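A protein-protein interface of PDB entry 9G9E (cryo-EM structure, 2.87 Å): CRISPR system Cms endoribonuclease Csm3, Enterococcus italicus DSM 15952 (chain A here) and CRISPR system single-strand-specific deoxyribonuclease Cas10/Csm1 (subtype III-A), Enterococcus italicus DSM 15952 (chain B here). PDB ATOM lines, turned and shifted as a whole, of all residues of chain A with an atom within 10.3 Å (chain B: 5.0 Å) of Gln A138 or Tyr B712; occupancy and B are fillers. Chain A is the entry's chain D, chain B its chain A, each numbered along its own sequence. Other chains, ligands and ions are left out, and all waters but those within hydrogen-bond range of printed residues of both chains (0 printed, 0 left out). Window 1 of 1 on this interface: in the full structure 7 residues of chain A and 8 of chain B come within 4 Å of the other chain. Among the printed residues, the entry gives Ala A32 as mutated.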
ATOM      1  N   HIS A  18      10.155 -24.718  20.179  1.00  0.00           N
ATOM      2  CA  HIS A  18      11.169 -25.410  20.974  1.00  0.00           C
ATOM      3  C   HIS A  18      10.490 -26.471  21.832  1.00  0.00           C
ATOM      4  O   HIS A  18       9.828 -26.146  22.820  1.00  0.00           O
ATOM      5  CB  HIS A  18      11.954 -24.430  21.839  1.00  0.00           C
ATOM      6  CG  HIS A  18      12.778 -25.091  22.901  1.00  0.00           C
ATOM      7  ND1 HIS A  18      13.890 -25.851  22.618  1.00  0.00           N
ATOM      8  CD2 HIS A  18      12.647 -25.104  24.249  1.00  0.00           C
ATOM      9  CE1 HIS A  18      14.411 -26.304  23.745  1.00  0.00           C
ATOM     10  NE2 HIS A  18      13.674 -25.866  24.748  1.00  0.00           N
ATOM     11  N   GLY A  29      25.396 -33.165  18.545  1.00  0.00           N
ATOM     12  CA  GLY A  29      26.394 -33.050  19.591  1.00  0.00           C
ATOM     13  C   GLY A  29      25.912 -32.270  20.797  1.00  0.00           C
ATOM     14  O   GLY A  29      24.750 -32.374  21.190  1.00  0.00           O
ATOM     15  N   ALA A  30      26.809 -31.484  21.388  1.00  0.00           N
ATOM     16  CA  ALA A  30      26.473 -30.672  22.553  1.00  0.00           C
ATOM     17  C   ALA A  30      25.785 -29.396  22.085  1.00  0.00           C
ATOM     18  O   ALA A  30      26.409 -28.541  21.448  1.00  0.00           O
ATOM     19  CB  ALA A  30      27.725 -30.358  23.366  1.00  0.00           C
ATOM     20  N   ILE A  31      24.498 -29.269  22.397  1.00  0.00           N
ATOM     21  CA  ILE A  31      23.693 -28.115  22.011  1.00  0.00           C
ATOM     22  C   ILE A  31      23.030 -27.556  23.262  1.00  0.00           C
ATOM     23  O   ILE A  31      22.567 -28.313  24.121  1.00  0.00           O
ATOM     24  CB  ILE A  31      22.634 -28.486  20.951  1.00  0.00           C
ATOM     25  CG1 ILE A  31      23.289 -29.181  19.756  1.00  0.00           C
ATOM     26  CG2 ILE A  31      21.875 -27.250  20.491  1.00  0.00           C
ATOM     27  CD1 ILE A  31      22.304 -29.650  18.707  1.00  0.00           C
ATOM     28  N   ALA A  32      22.992 -26.229  23.365  1.00  0.00           N
ATOM     29  CA  ALA A  32      22.353 -25.564  24.496  1.00  0.00           C
ATOM     30  C   ALA A  32      20.843 -25.594  24.294  1.00  0.00           C
ATOM     31  O   ALA A  32      20.323 -24.963  23.367  1.00  0.00           O
ATOM     32  CB  ALA A  32      22.864 -24.134  24.635  1.00  0.00           C
ATOM     33  N   SER A  33      20.143 -26.324  25.165  1.00  0.00           N
ATOM     34  CA  SER A  33      18.700 -26.531  25.092  1.00  0.00           C
ATOM     35  C   SER A  33      18.297 -27.063  23.720  1.00  0.00           C
ATOM     36  O   SER A  33      17.615 -26.363  22.960  1.00  0.00           O
ATOM     37  CB  SER A  33      17.950 -25.233  25.400  1.00  0.00           C
ATOM     38  OG  SER A  33      18.077 -24.885  26.768  1.00  0.00           O
ATOM     39  N   PRO A  34      18.695 -28.282  23.365  1.00  0.00           N
ATOM     40  CA  PRO A  34      18.353 -28.812  22.044  1.00  0.00           C
ATOM     41  C   PRO A  34      16.884 -29.197  21.953  1.00  0.00           C
ATOM     42  O   PRO A  34      16.204 -29.424  22.955  1.00  0.00           O
ATOM     43  CB  PRO A  34      19.255 -30.040  21.912  1.00  0.00           C
ATOM     44  CG  PRO A  34      19.446 -30.497  23.312  1.00  0.00           C
ATOM     45  CD  PRO A  34      19.457 -29.256  24.168  1.00  0.00           C
ATOM     46  N   VAL A  35      16.399 -29.263  20.719  1.00  0.00           N
ATOM     47  CA  VAL A  35      15.039 -29.702  20.452  1.00  0.00           C
ATOM     48  C   VAL A  35      15.036 -31.210  20.230  1.00  0.00           C
ATOM     49  O   VAL A  35      16.066 -31.828  19.949  1.00  0.00           O
ATOM     50  CB  VAL A  35      14.427 -28.963  19.245  1.00  0.00           C
ATOM     51  CG1 VAL A  35      14.126 -27.520  19.605  1.00  0.00           C
ATOM     52  CG2 VAL A  35      15.360 -29.036  18.048  1.00  0.00           C
ATOM     53  N   ARG A  42      17.871 -37.179  12.093  1.00  0.00           N
ATOM     54  CA  ARG A  42      18.278 -35.983  12.833  1.00  0.00           C
ATOM     55  C   ARG A  42      17.474 -34.761  12.394  1.00  0.00           C
ATOM     56  O   ARG A  42      18.003 -33.655  12.266  1.00  0.00           O
ATOM     57  CB  ARG A  42      19.782 -35.728  12.697  1.00  0.00           C
ATOM     58  CG  ARG A  42      20.413 -35.128  13.940  1.00  0.00           C
ATOM     59  CD  ARG A  42      21.729 -34.427  13.629  1.00  0.00           C
ATOM     60  NE  ARG A  42      22.058 -33.380  14.591  1.00  0.00           N
ATOM     61  CZ  ARG A  42      22.246 -33.566  15.892  1.00  0.00           C
ATOM     62  NH1 ARG A  42      22.200 -34.771  16.436  1.00  0.00           N
ATOM     63  NH2 ARG A  42      22.502 -32.515  16.665  1.00  0.00           N
ATOM     64  N   GLU A 120      17.230 -22.944  14.479  1.00  0.00           N
ATOM     65  CA  GLU A 120      17.900 -21.692  14.789  1.00  0.00           C
ATOM     66  C   GLU A 120      18.263 -21.645  16.267  1.00  0.00           C
ATOM     67  O   GLU A 120      17.683 -22.352  17.096  1.00  0.00           O
ATOM     68  CB  GLU A 120      17.014 -20.493  14.435  1.00  0.00           C
ATOM     69  CG  GLU A 120      15.589 -20.613  14.948  1.00  0.00           C
ATOM     70  CD  GLU A 120      14.868 -19.281  14.987  1.00  0.00           C
ATOM     71  OE1 GLU A 120      15.425 -18.319  15.558  1.00  0.00           O
ATOM     72  OE2 GLU A 120      13.744 -19.197  14.449  1.00  0.00           O
ATOM     73  N   THR A 121      19.237 -20.802  16.588  1.00  0.00           N
ATOM     74  CA  THR A 121      19.675 -20.585  17.961  1.00  0.00           C
ATOM     75  C   THR A 121      19.196 -19.214  18.414  1.00  0.00           C
ATOM     76  O   THR A 121      19.508 -18.202  17.776  1.00  0.00           O
ATOM     77  CB  THR A 121      21.196 -20.690  18.080  1.00  0.00           C
ATOM     78  OG1 THR A 121      21.634 -21.942  17.539  1.00  0.00           O
ATOM     79  CG2 THR A 121      21.620 -20.599  19.537  1.00  0.00           C
ATOM     80  N   LYS A 122      18.441 -19.183  19.506  1.00  0.00           N
ATOM     81  CA  LYS A 122      17.915 -17.946  20.064  1.00  0.00           C
ATOM     82  C   LYS A 122      18.681 -17.591  21.331  1.00  0.00           C
ATOM     83  O   LYS A 122      18.852 -18.433  22.221  1.00  0.00           O
ATOM     84  CB  LYS A 122      16.422 -18.068  20.367  1.00  0.00           C
ATOM     85  CG  LYS A 122      15.750 -16.740  20.675  1.00  0.00           C
ATOM     86  CD  LYS A 122      14.434 -16.938  21.403  1.00  0.00           C
ATOM     87  CE  LYS A 122      13.683 -15.624  21.542  1.00  0.00           C
ATOM     88  NZ  LYS A 122      14.557 -14.538  22.062  1.00  0.00           N
ATOM     89  N   PHE A 123      19.137 -16.345  21.400  1.00  0.00           N
ATOM     90  CA  PHE A 123      19.876 -15.826  22.541  1.00  0.00           C
ATOM     91  C   PHE A 123      18.944 -14.960  23.378  1.00  0.00           C
ATOM     92  O   PHE A 123      18.280 -14.065  22.846  1.00  0.00           O
ATOM     93  CB  PHE A 123      21.083 -15.008  22.079  1.00  0.00           C
ATOM     94  CG  PHE A 123      22.079 -15.790  21.268  1.00  0.00           C
ATOM     95  CD1 PHE A 123      21.868 -16.017  19.918  1.00  0.00           C
ATOM     96  CD2 PHE A 123      23.232 -16.284  21.852  1.00  0.00           C
ATOM     97  CE1 PHE A 123      22.783 -16.733  19.168  1.00  0.00           C
ATOM     98  CE2 PHE A 123      24.152 -16.999  21.106  1.00  0.00           C
ATOM     99  CZ  PHE A 123      23.926 -17.224  19.764  1.00  0.00           C
ATOM    100  N   GLU A 124      18.895 -15.225  24.681  1.00  0.00           N
ATOM    101  CA  GLU A 124      18.027 -14.486  25.581  1.00  0.00           C
ATOM    102  C   GLU A 124      18.822 -14.010  26.783  1.00  0.00           C
ATOM    103  O   GLU A 124      19.866 -14.572  27.122  1.00  0.00           O
ATOM    104  CB  GLU A 124      16.839 -15.327  26.060  1.00  0.00           C
ATOM    105  CG  GLU A 124      15.734 -15.489  25.038  1.00  0.00           C
ATOM    106  CD  GLU A 124      15.360 -16.935  24.821  1.00  0.00           C
ATOM    107  OE1 GLU A 124      14.165 -17.206  24.578  1.00  0.00           O
ATOM    108  OE2 GLU A 124      16.258 -17.799  24.898  1.00  0.00           O
ATOM    109  N   ASN A 125      18.317 -12.962  27.421  1.00  0.00           N
ATOM    110  CA  ASN A 125      18.887 -12.422  28.641  1.00  0.00           C
ATOM    111  C   ASN A 125      17.958 -12.695  29.815  1.00  0.00           C
ATOM    112  O   ASN A 125      16.778 -13.007  29.646  1.00  0.00           O
ATOM    113  CB  ASN A 125      19.134 -10.915  28.516  1.00  0.00           C
ATOM    114  CG  ASN A 125      20.568 -10.587  28.172  1.00  0.00           C
ATOM    115  OD1 ASN A 125      21.434 -11.461  28.170  1.00  0.00           O
ATOM    116  ND2 ASN A 125      20.830  -9.320  27.879  1.00  0.00           N
ATOM    117  N   THR A 126      18.524 -12.603  31.014  1.00  0.00           N
ATOM    118  CA  THR A 126      17.750 -12.562  32.251  1.00  0.00           C
ATOM    119  C   THR A 126      18.379 -11.499  33.138  1.00  0.00           C
ATOM    120  O   THR A 126      19.466 -11.709  33.682  1.00  0.00           O
ATOM    121  CB  THR A 126      17.728 -13.920  32.951  1.00  0.00           C
ATOM    122  OG1 THR A 126      17.065 -14.875  32.116  1.00  0.00           O
ATOM    123  CG2 THR A 126      16.994 -13.819  34.278  1.00  0.00           C
ATOM    124  N   ASN A 135      22.097 -12.371  32.732  1.00  0.00           N
ATOM    125  CA  ASN A 135      22.604 -13.716  32.519  1.00  0.00           C
ATOM    126  C   ASN A 135      22.163 -14.194  31.148  1.00  0.00           C
ATOM    127  O   ASN A 135      20.952 -14.202  30.871  1.00  0.00           O
ATOM    128  CB  ASN A 135      22.087 -14.659  33.599  1.00  0.00           C
ATOM    129  CG  ASN A 135      22.697 -16.043  33.511  1.00  0.00           C
ATOM    130  OD1 ASN A 135      23.792 -16.220  32.978  1.00  0.00           O
ATOM    131  ND2 ASN A 135      21.987 -17.036  34.032  1.00  0.00           N
ATOM    132  N   PRO A 136      23.080 -14.557  30.257  1.00  0.00           N
ATOM    133  CA  PRO A 136      22.681 -15.045  28.933  1.00  0.00           C
ATOM    134  C   PRO A 136      22.213 -16.492  28.972  1.00  0.00           C
ATOM    135  O   PRO A 136      22.538 -17.262  29.878  1.00  0.00           O
ATOM    136  CB  PRO A 136      23.963 -14.903  28.109  1.00  0.00           C
ATOM    137  CG  PRO A 136      25.056 -15.057  29.108  1.00  0.00           C
ATOM    138  CD  PRO A 136      24.544 -14.457  30.393  1.00  0.00           C
ATOM    139  N   ARG A 137      21.434 -16.853  27.954  1.00  0.00           N
ATOM    140  CA  ARG A 137      20.908 -18.206  27.835  1.00  0.00           C
ATOM    141  C   ARG A 137      20.631 -18.503  26.370  1.00  0.00           C
ATOM    142  O   ARG A 137      20.034 -17.682  25.669  1.00  0.00           O
ATOM    143  CB  ARG A 137      19.633 -18.375  28.670  1.00  0.00           C
ATOM    144  CG  ARG A 137      18.692 -19.459  28.168  1.00  0.00           C
ATOM    145  CD  ARG A 137      17.430 -19.545  29.014  1.00  0.00           C
ATOM    146  NE  ARG A 137      16.414 -18.577  28.614  1.00  0.00           N
ATOM    147  CZ  ARG A 137      16.287 -17.363  29.131  1.00  0.00           C
ATOM    148  NH1 ARG A 137      17.113 -16.919  30.064  1.00  0.00           N
ATOM    149  NH2 ARG A 137      15.304 -16.576  28.706  1.00  0.00           N
ATOM    150  N   GLN A 138      21.062 -19.672  25.912  1.00  0.00           N
ATOM    151  CA  GLN A 138      20.849 -20.098  24.537  1.00  0.00           C
ATOM    152  C   GLN A 138      19.792 -21.192  24.483  1.00  0.00           C
ATOM    153  O   GLN A 138      19.817 -22.133  25.281  1.00  0.00           O
ATOM    154  CB  GLN A 138      22.148 -20.610  23.915  1.00  0.00           C
ATOM    155  CG  GLN A 138      22.839 -19.622  23.003  1.00  0.00           C
ATOM    156  CD  GLN A 138      24.256 -20.039  22.669  1.00  0.00           C
ATOM    157  OE1 GLN A 138      24.607 -20.208  21.502  1.00  0.00           O
ATOM    158  NE2 GLN A 138      25.078 -20.213  23.697  1.00  0.00           N
ATOM    159  N   ILE A 139      18.862 -21.065  23.538  1.00  0.00           N
ATOM    160  CA  ILE A 139      17.905 -22.128  23.264  1.00  0.00           C
ATOM    161  C   ILE A 139      17.933 -22.420  21.772  1.00  0.00           C
ATOM    162  O   ILE A 139      18.471 -21.655  20.972  1.00  0.00           O
ATOM    163  CB  ILE A 139      16.471 -21.787  23.716  1.00  0.00           C
ATOM    164  CG1 ILE A 139      16.003 -20.480  23.082  1.00  0.00           C
ATOM    165  CG2 ILE A 139      16.393 -21.705  25.233  1.00  0.00           C
ATOM    166  CD1 ILE A 139      14.574 -20.131  23.419  1.00  0.00           C
ATOM    167  N   GLU A 140      17.345 -23.552  21.404  1.00  0.00           N
ATOM    168  CA  GLU A 140      17.212 -23.949  20.013  1.00  0.00           C
ATOM    169  C   GLU A 140      15.737 -24.018  19.644  1.00  0.00           C
ATOM    170  O   GLU A 140      14.917 -24.508  20.424  1.00  0.00           O
ATOM    171  CB  GLU A 140      17.883 -25.300  19.760  1.00  0.00           C
ATOM    172  CG  GLU A 140      18.074 -25.631  18.295  1.00  0.00           C
ATOM    173  CD  GLU A 140      18.653 -27.012  18.090  1.00  0.00           C
ATOM    174  OE1 GLU A 140      18.347 -27.907  18.904  1.00  0.00           O
ATOM    175  OE2 GLU A 140      19.419 -27.201  17.123  1.00  0.00           O
ATOM    176  N   ARG A 141      15.403 -23.516  18.461  1.00  0.00           N
ATOM    177  CA  ARG A 141      14.031 -23.512  17.980  1.00  0.00           C
ATOM    178  C   ARG A 141      13.987 -24.034  16.552  1.00  0.00           C
ATOM    179  O   ARG A 141      15.009 -24.132  15.873  1.00  0.00           O
ATOM    180  CB  ARG A 141      13.408 -22.110  18.028  1.00  0.00           C
ATOM    181  CG  ARG A 141      13.529 -21.398  19.359  1.00  0.00           C
ATOM    182  CD  ARG A 141      13.597 -19.898  19.151  1.00  0.00           C
ATOM    183  NE  ARG A 141      12.276 -19.310  18.971  1.00  0.00           N
ATOM    184  CZ  ARG A 141      12.055 -18.120  18.429  1.00  0.00           C
ATOM    185  NH1 ARG A 141      13.049 -17.359  18.002  1.00  0.00           N
ATOM    186  NH2 ARG A 141      10.805 -17.684  18.310  1.00  0.00           N
ATOM    187  N   ASN A 189       7.155 -18.103  21.703  1.00  0.00           N
ATOM    188  CA  ASN A 189       7.647 -19.340  21.116  1.00  0.00           C
ATOM    189  C   ASN A 189       6.490 -20.298  20.869  1.00  0.00           C
ATOM    190  O   ASN A 189       5.446 -20.221  21.522  1.00  0.00           O
ATOM    191  CB  ASN A 189       8.683 -20.021  22.019  1.00  0.00           C
ATOM    192  CG  ASN A 189      10.054 -19.386  21.921  1.00  0.00           C
ATOM    193  OD1 ASN A 189      10.310 -18.567  21.042  1.00  0.00           O
ATOM    194  ND2 ASN A 189      10.948 -19.767  22.826  1.00  0.00           N
ATOM    195  N   GLY B 707      34.171 -19.329  26.837  1.00  0.00           N
ATOM    196  CA  GLY B 707      34.034 -19.757  25.463  1.00  0.00           C
ATOM    197  C   GLY B 707      32.914 -20.735  25.199  1.00  0.00           C
ATOM    198  O   GLY B 707      32.976 -21.461  24.204  1.00  0.00           O
ATOM    199  N   LYS B 708      31.891 -20.780  26.057  1.00  0.00           N
ATOM    200  CA  LYS B 708      30.804 -21.737  25.866  1.00  0.00           C
ATOM    201  C   LYS B 708      30.066 -21.478  24.556  1.00  0.00           C
ATOM    202  O   LYS B 708      29.863 -22.396  23.752  1.00  0.00           O
ATOM    203  CB  LYS B 708      29.840 -21.671  27.052  1.00  0.00           C
ATOM    204  CG  LYS B 708      28.872 -22.839  27.135  1.00  0.00           C
ATOM    205  CD  LYS B 708      27.689 -22.517  28.036  1.00  0.00           C
ATOM    206  CE  LYS B 708      28.112 -22.392  29.491  1.00  0.00           C
ATOM    207  NZ  LYS B 708      26.946 -22.154  30.388  1.00  0.00           N
ATOM    208  N   SER B 709      29.662 -20.227  24.322  1.00  0.00           N
ATOM    209  CA  SER B 709      28.949 -19.895  23.094  1.00  0.00           C
ATOM    210  C   SER B 709      29.831 -20.084  21.866  1.00  0.00           C
ATOM    211  O   SER B 709      29.364 -20.566  20.828  1.00  0.00           O
ATOM    212  CB  SER B 709      28.427 -18.460  23.161  1.00  0.00           C
ATOM    213  OG  SER B 709      27.571 -18.279  24.275  1.00  0.00           O
ATOM    214  N   PHE B 710      31.105 -19.701  21.960  1.00  0.00           N
ATOM    215  CA  PHE B 710      32.008 -19.845  20.823  1.00  0.00           C
ATOM    216  C   PHE B 710      32.264 -21.317  20.517  1.00  0.00           C
ATOM    217  O   PHE B 710      32.336 -21.714  19.348  1.00  0.00           O
ATOM    218  CB  PHE B 710      33.306 -19.083  21.103  1.00  0.00           C
ATOM    219  CG  PHE B 710      34.515 -19.622  20.390  1.00  0.00           C
ATOM    220  CD1 PHE B 710      34.593 -19.586  19.007  1.00  0.00           C
ATOM    221  CD2 PHE B 710      35.591 -20.116  21.103  1.00  0.00           C
ATOM    222  CE1 PHE B 710      35.706 -20.064  18.349  1.00  0.00           C
ATOM    223  CE2 PHE B 710      36.711 -20.590  20.448  1.00  0.00           C
ATOM    224  CZ  PHE B 710      36.769 -20.558  19.070  1.00  0.00           C
ATOM    225  N   LEU B 711      32.380 -22.147  21.557  1.00  0.00           N
ATOM    226  CA  LEU B 711      32.478 -23.588  21.347  1.00  0.00           C
ATOM    227  C   LEU B 711      31.207 -24.146  20.716  1.00  0.00           C
ATOM    228  O   LEU B 711      31.270 -25.052  19.876  1.00  0.00           O
ATOM    229  CB  LEU B 711      32.768 -24.299  22.669  1.00  0.00           C
ATOM    230  CG  LEU B 711      34.171 -24.191  23.269  1.00  0.00           C
ATOM    231  CD1 LEU B 711      34.198 -24.769  24.675  1.00  0.00           C
ATOM    232  CD2 LEU B 711      35.178 -24.892  22.387  1.00  0.00           C
ATOM    233  N   TYR B 712      30.042 -23.631  21.118  1.00  0.00           N
ATOM    234  CA  TYR B 712      28.792 -24.062  20.498  1.00  0.00           C
ATOM    235  C   TYR B 712      28.761 -23.713  19.015  1.00  0.00           C
ATOM    236  O   TYR B 712      28.326 -24.522  18.187  1.00  0.00           O
ATOM    237  CB  TYR B 712      27.602 -23.429  21.217  1.00  0.00           C
ATOM    238  CG  TYR B 712      27.234 -24.110  22.513  1.00  0.00           C
ATOM    239  CD1 TYR B 712      27.333 -25.487  22.646  1.00  0.00           C
ATOM    240  CD2 TYR B 712      26.780 -23.375  23.598  1.00  0.00           C
ATOM    241  CE1 TYR B 712      26.995 -26.115  23.827  1.00  0.00           C
ATOM    242  CE2 TYR B 712      26.438 -23.994  24.784  1.00  0.00           C
ATOM    243  CZ  TYR B 712      26.548 -25.364  24.892  1.00  0.00           C
ATOM    244  OH  TYR B 712      26.209 -25.987  26.071  1.00  0.00           O
ATOM    245  N   LYS B 713      29.210 -22.506  18.665  1.00  0.00           N
ATOM    246  CA  LYS B 713      29.302 -22.134  17.256  1.00  0.00           C
ATOM    247  C   LYS B 713      30.286 -23.027  16.510  1.00  0.00           C
ATOM    248  O   LYS B 713      30.038 -23.408  15.360  1.00  0.00           O
ATOM    249  CB  LYS B 713      29.695 -20.663  17.111  1.00  0.00           C
ATOM    250  CG  LYS B 713      28.847 -19.701  17.923  1.00  0.00           C
ATOM    251  CD  LYS B 713      28.978 -18.274  17.414  1.00  0.00           C
ATOM    252  CE  LYS B 713      29.184 -17.301  18.566  1.00  0.00           C
ATOM    253  NZ  LYS B 713      30.602 -16.863  18.696  1.00  0.00           N
ATOM    254  N   MET B 714      31.413 -23.367  17.144  1.00  0.00           N
ATOM    255  CA  MET B 714      32.358 -24.281  16.508  1.00  0.00           C
ATOM    256  C   MET B 714      31.722 -25.640  16.249  1.00  0.00           C
ATOM    257  O   MET B 714      31.919 -26.230  15.184  1.00  0.00           O
ATOM    258  CB  MET B 714      33.620 -24.451  17.354  1.00  0.00           C
ATOM    259  CG  MET B 714      34.680 -23.388  17.138  1.00  0.00           C
ATOM    260  SD  MET B 714      36.341 -24.048  17.400  1.00  0.00           S
ATOM    261  CE  MET B 714      36.518 -23.909  19.172  1.00  0.00           C
ATOM    262  N   LEU B 715      30.964 -26.158  17.218  1.00  0.00           N
ATOM    263  CA  LEU B 715      30.277 -27.432  17.018  1.00  0.00           C
ATOM    264  C   LEU B 715      29.256 -27.340  15.891  1.00  0.00           C
ATOM    265  O   LEU B 715      29.152 -28.250  15.058  1.00  0.00           O
ATOM    266  CB  LEU B 715      29.598 -27.875  18.314  1.00  0.00           C
ATOM    267  CG  LEU B 715      30.478 -28.608  19.324  1.00  0.00           C
ATOM    268  CD1 LEU B 715      29.715 -28.867  20.608  1.00  0.00           C
ATOM    269  CD2 LEU B 715      30.996 -29.911  18.736  1.00  0.00           C
ATOM    270  N   GLU B 716      28.498 -26.241  15.847  1.00  0.00           N
ATOM    271  CA  GLU B 716      27.513 -26.058  14.788  1.00  0.00           C
ATOM    272  C   GLU B 716      28.179 -26.029  13.418  1.00  0.00           C
ATOM    273  O   GLU B 716      27.679 -26.632  12.462  1.00  0.00           O
ATOM    274  CB  GLU B 716      26.723 -24.770  15.022  1.00  0.00           C
ATOM    275  CG  GLU B 716      25.409 -24.961  15.760  1.00  0.00           C
ATOM    276  CD  GLU B 716      25.006 -23.736  16.562  1.00  0.00           C
ATOM    277  OE1 GLU B 716      25.004 -23.811  17.808  1.00  0.00           O
ATOM    278  OE2 GLU B 716      24.692 -22.697  15.944  1.00  0.00           O
ATOM    279  N   VAL B 767      33.154 -28.468  26.376  1.00  0.00           N
ATOM    280  CA  VAL B 767      31.836 -27.905  26.654  1.00  0.00           C
ATOM    281  C   VAL B 767      31.239 -28.541  27.901  1.00  0.00           C
ATOM    282  O   VAL B 767      30.670 -27.853  28.758  1.00  0.00           O
ATOM    283  CB  VAL B 767      30.912 -28.081  25.433  1.00  0.00           C
ATOM    284  CG1 VAL B 767      29.455 -27.899  25.831  1.00  0.00           C
ATOM    285  CG2 VAL B 767      31.288 -27.101  24.338  1.00  0.00           C
ATOM    286  N   ARG B 771      30.279 -26.151  32.207  1.00  0.00           N
ATOM    287  CA  ARG B 771      28.822 -26.135  32.153  1.00  0.00           C
ATOM    288  C   ARG B 771      28.293 -26.183  33.580  1.00  0.00           C
ATOM    289  O   ARG B 771      29.057 -26.250  34.546  1.00  0.00           O
ATOM    290  CB  ARG B 771      28.276 -27.294  31.312  1.00  0.00           C
ATOM    291  CG  ARG B 771      27.780 -26.880  29.934  1.00  0.00           C
ATOM    292  CD  ARG B 771      27.032 -28.004  29.234  1.00  0.00           C
ATOM    293  NE  ARG B 771      25.678 -28.168  29.751  1.00  0.00           N
ATOM    294  CZ  ARG B 771      24.735 -28.892  29.164  1.00  0.00           C
ATOM    295  NH1 ARG B 771      24.965 -29.539  28.033  1.00  0.00           N
ATOM    296  NH2 ARG B 771      23.532 -28.969  29.725  1.00  0.00           N
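Printed residues of chain A that touch a printed residue of chain B: Ala A30, Ala A32, Thr A121 and Gln A138.
Hydrophobic or aromatic side chains of chain A that line the printed part of chain B: Ala A30 and Ala A32.
Of the 12 printed residues of chain B, 5 touch a printed residue of chain A.
Printed residues of chain B that touch a printed residue of chain A: Ser B709, Tyr B712, Leu B715, Glu B716 and Val B767.
Among the printed residues, 7 pairs touch across the chains.
Among the printed residues, no Asp or Glu carboxylate lies within 4 Å of a Lys or Arg side-chain nitrogen of the other chain.
Among the printed residues, merely in contact across the chains: Ala A30 with Tyr B712 (3.4 Å), Ala A30 with Leu B715 (3.4 Å), Ala A30 with Val B767 (3.9 Å), Ala A32 with Tyr B712 (3.6 Å), Thr A121 with Glu B716 (3.5 Å) and Gln A138 with Tyr B712 (3.6 Å).
Of chain B, only Ser B709 (3.2 Å) and Tyr B712 (3.6 Å) come within 4 Å of Gln A138.
Of chain A, only Ala A30, Ala A32 and Gln A138 come within 4 Å of Tyr B712.
Ser B709 touches just one residue of chain A: Gln A138 (3.2 Å).
Glu B716 touches just one residue of chain A: Thr A121.
Printed residues of chain B within 4 Å of Ala A30: Tyr B712, Leu B715 and Val B767.
Printed residues of chain A within 4 Å of Val B767: Ala A30.
Of the printed residues of chain B, Thr A121 touches Glu B716 (3.5 Å).
Asn A189 touches none of the printed residues of chain B.
Arg A141 touches none of the printed residues of chain B.
The nearest printed residue of chain B that does not touch Gln A138 is Glu B716 (5.2 Å).
The nearest residue of chain A that does not touch Tyr B712 is Ile A31 (4.3 Å).
The nearest printed residue of chain A that does not touch Val B767 is Ile A31 (6.2 Å).
The side-chain amide nitrogen (NE2) of Gln A138 sits at hydrogen-bond distance from the side-chain hydroxyl (OG) of Ser B709, 3.2 Å away.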
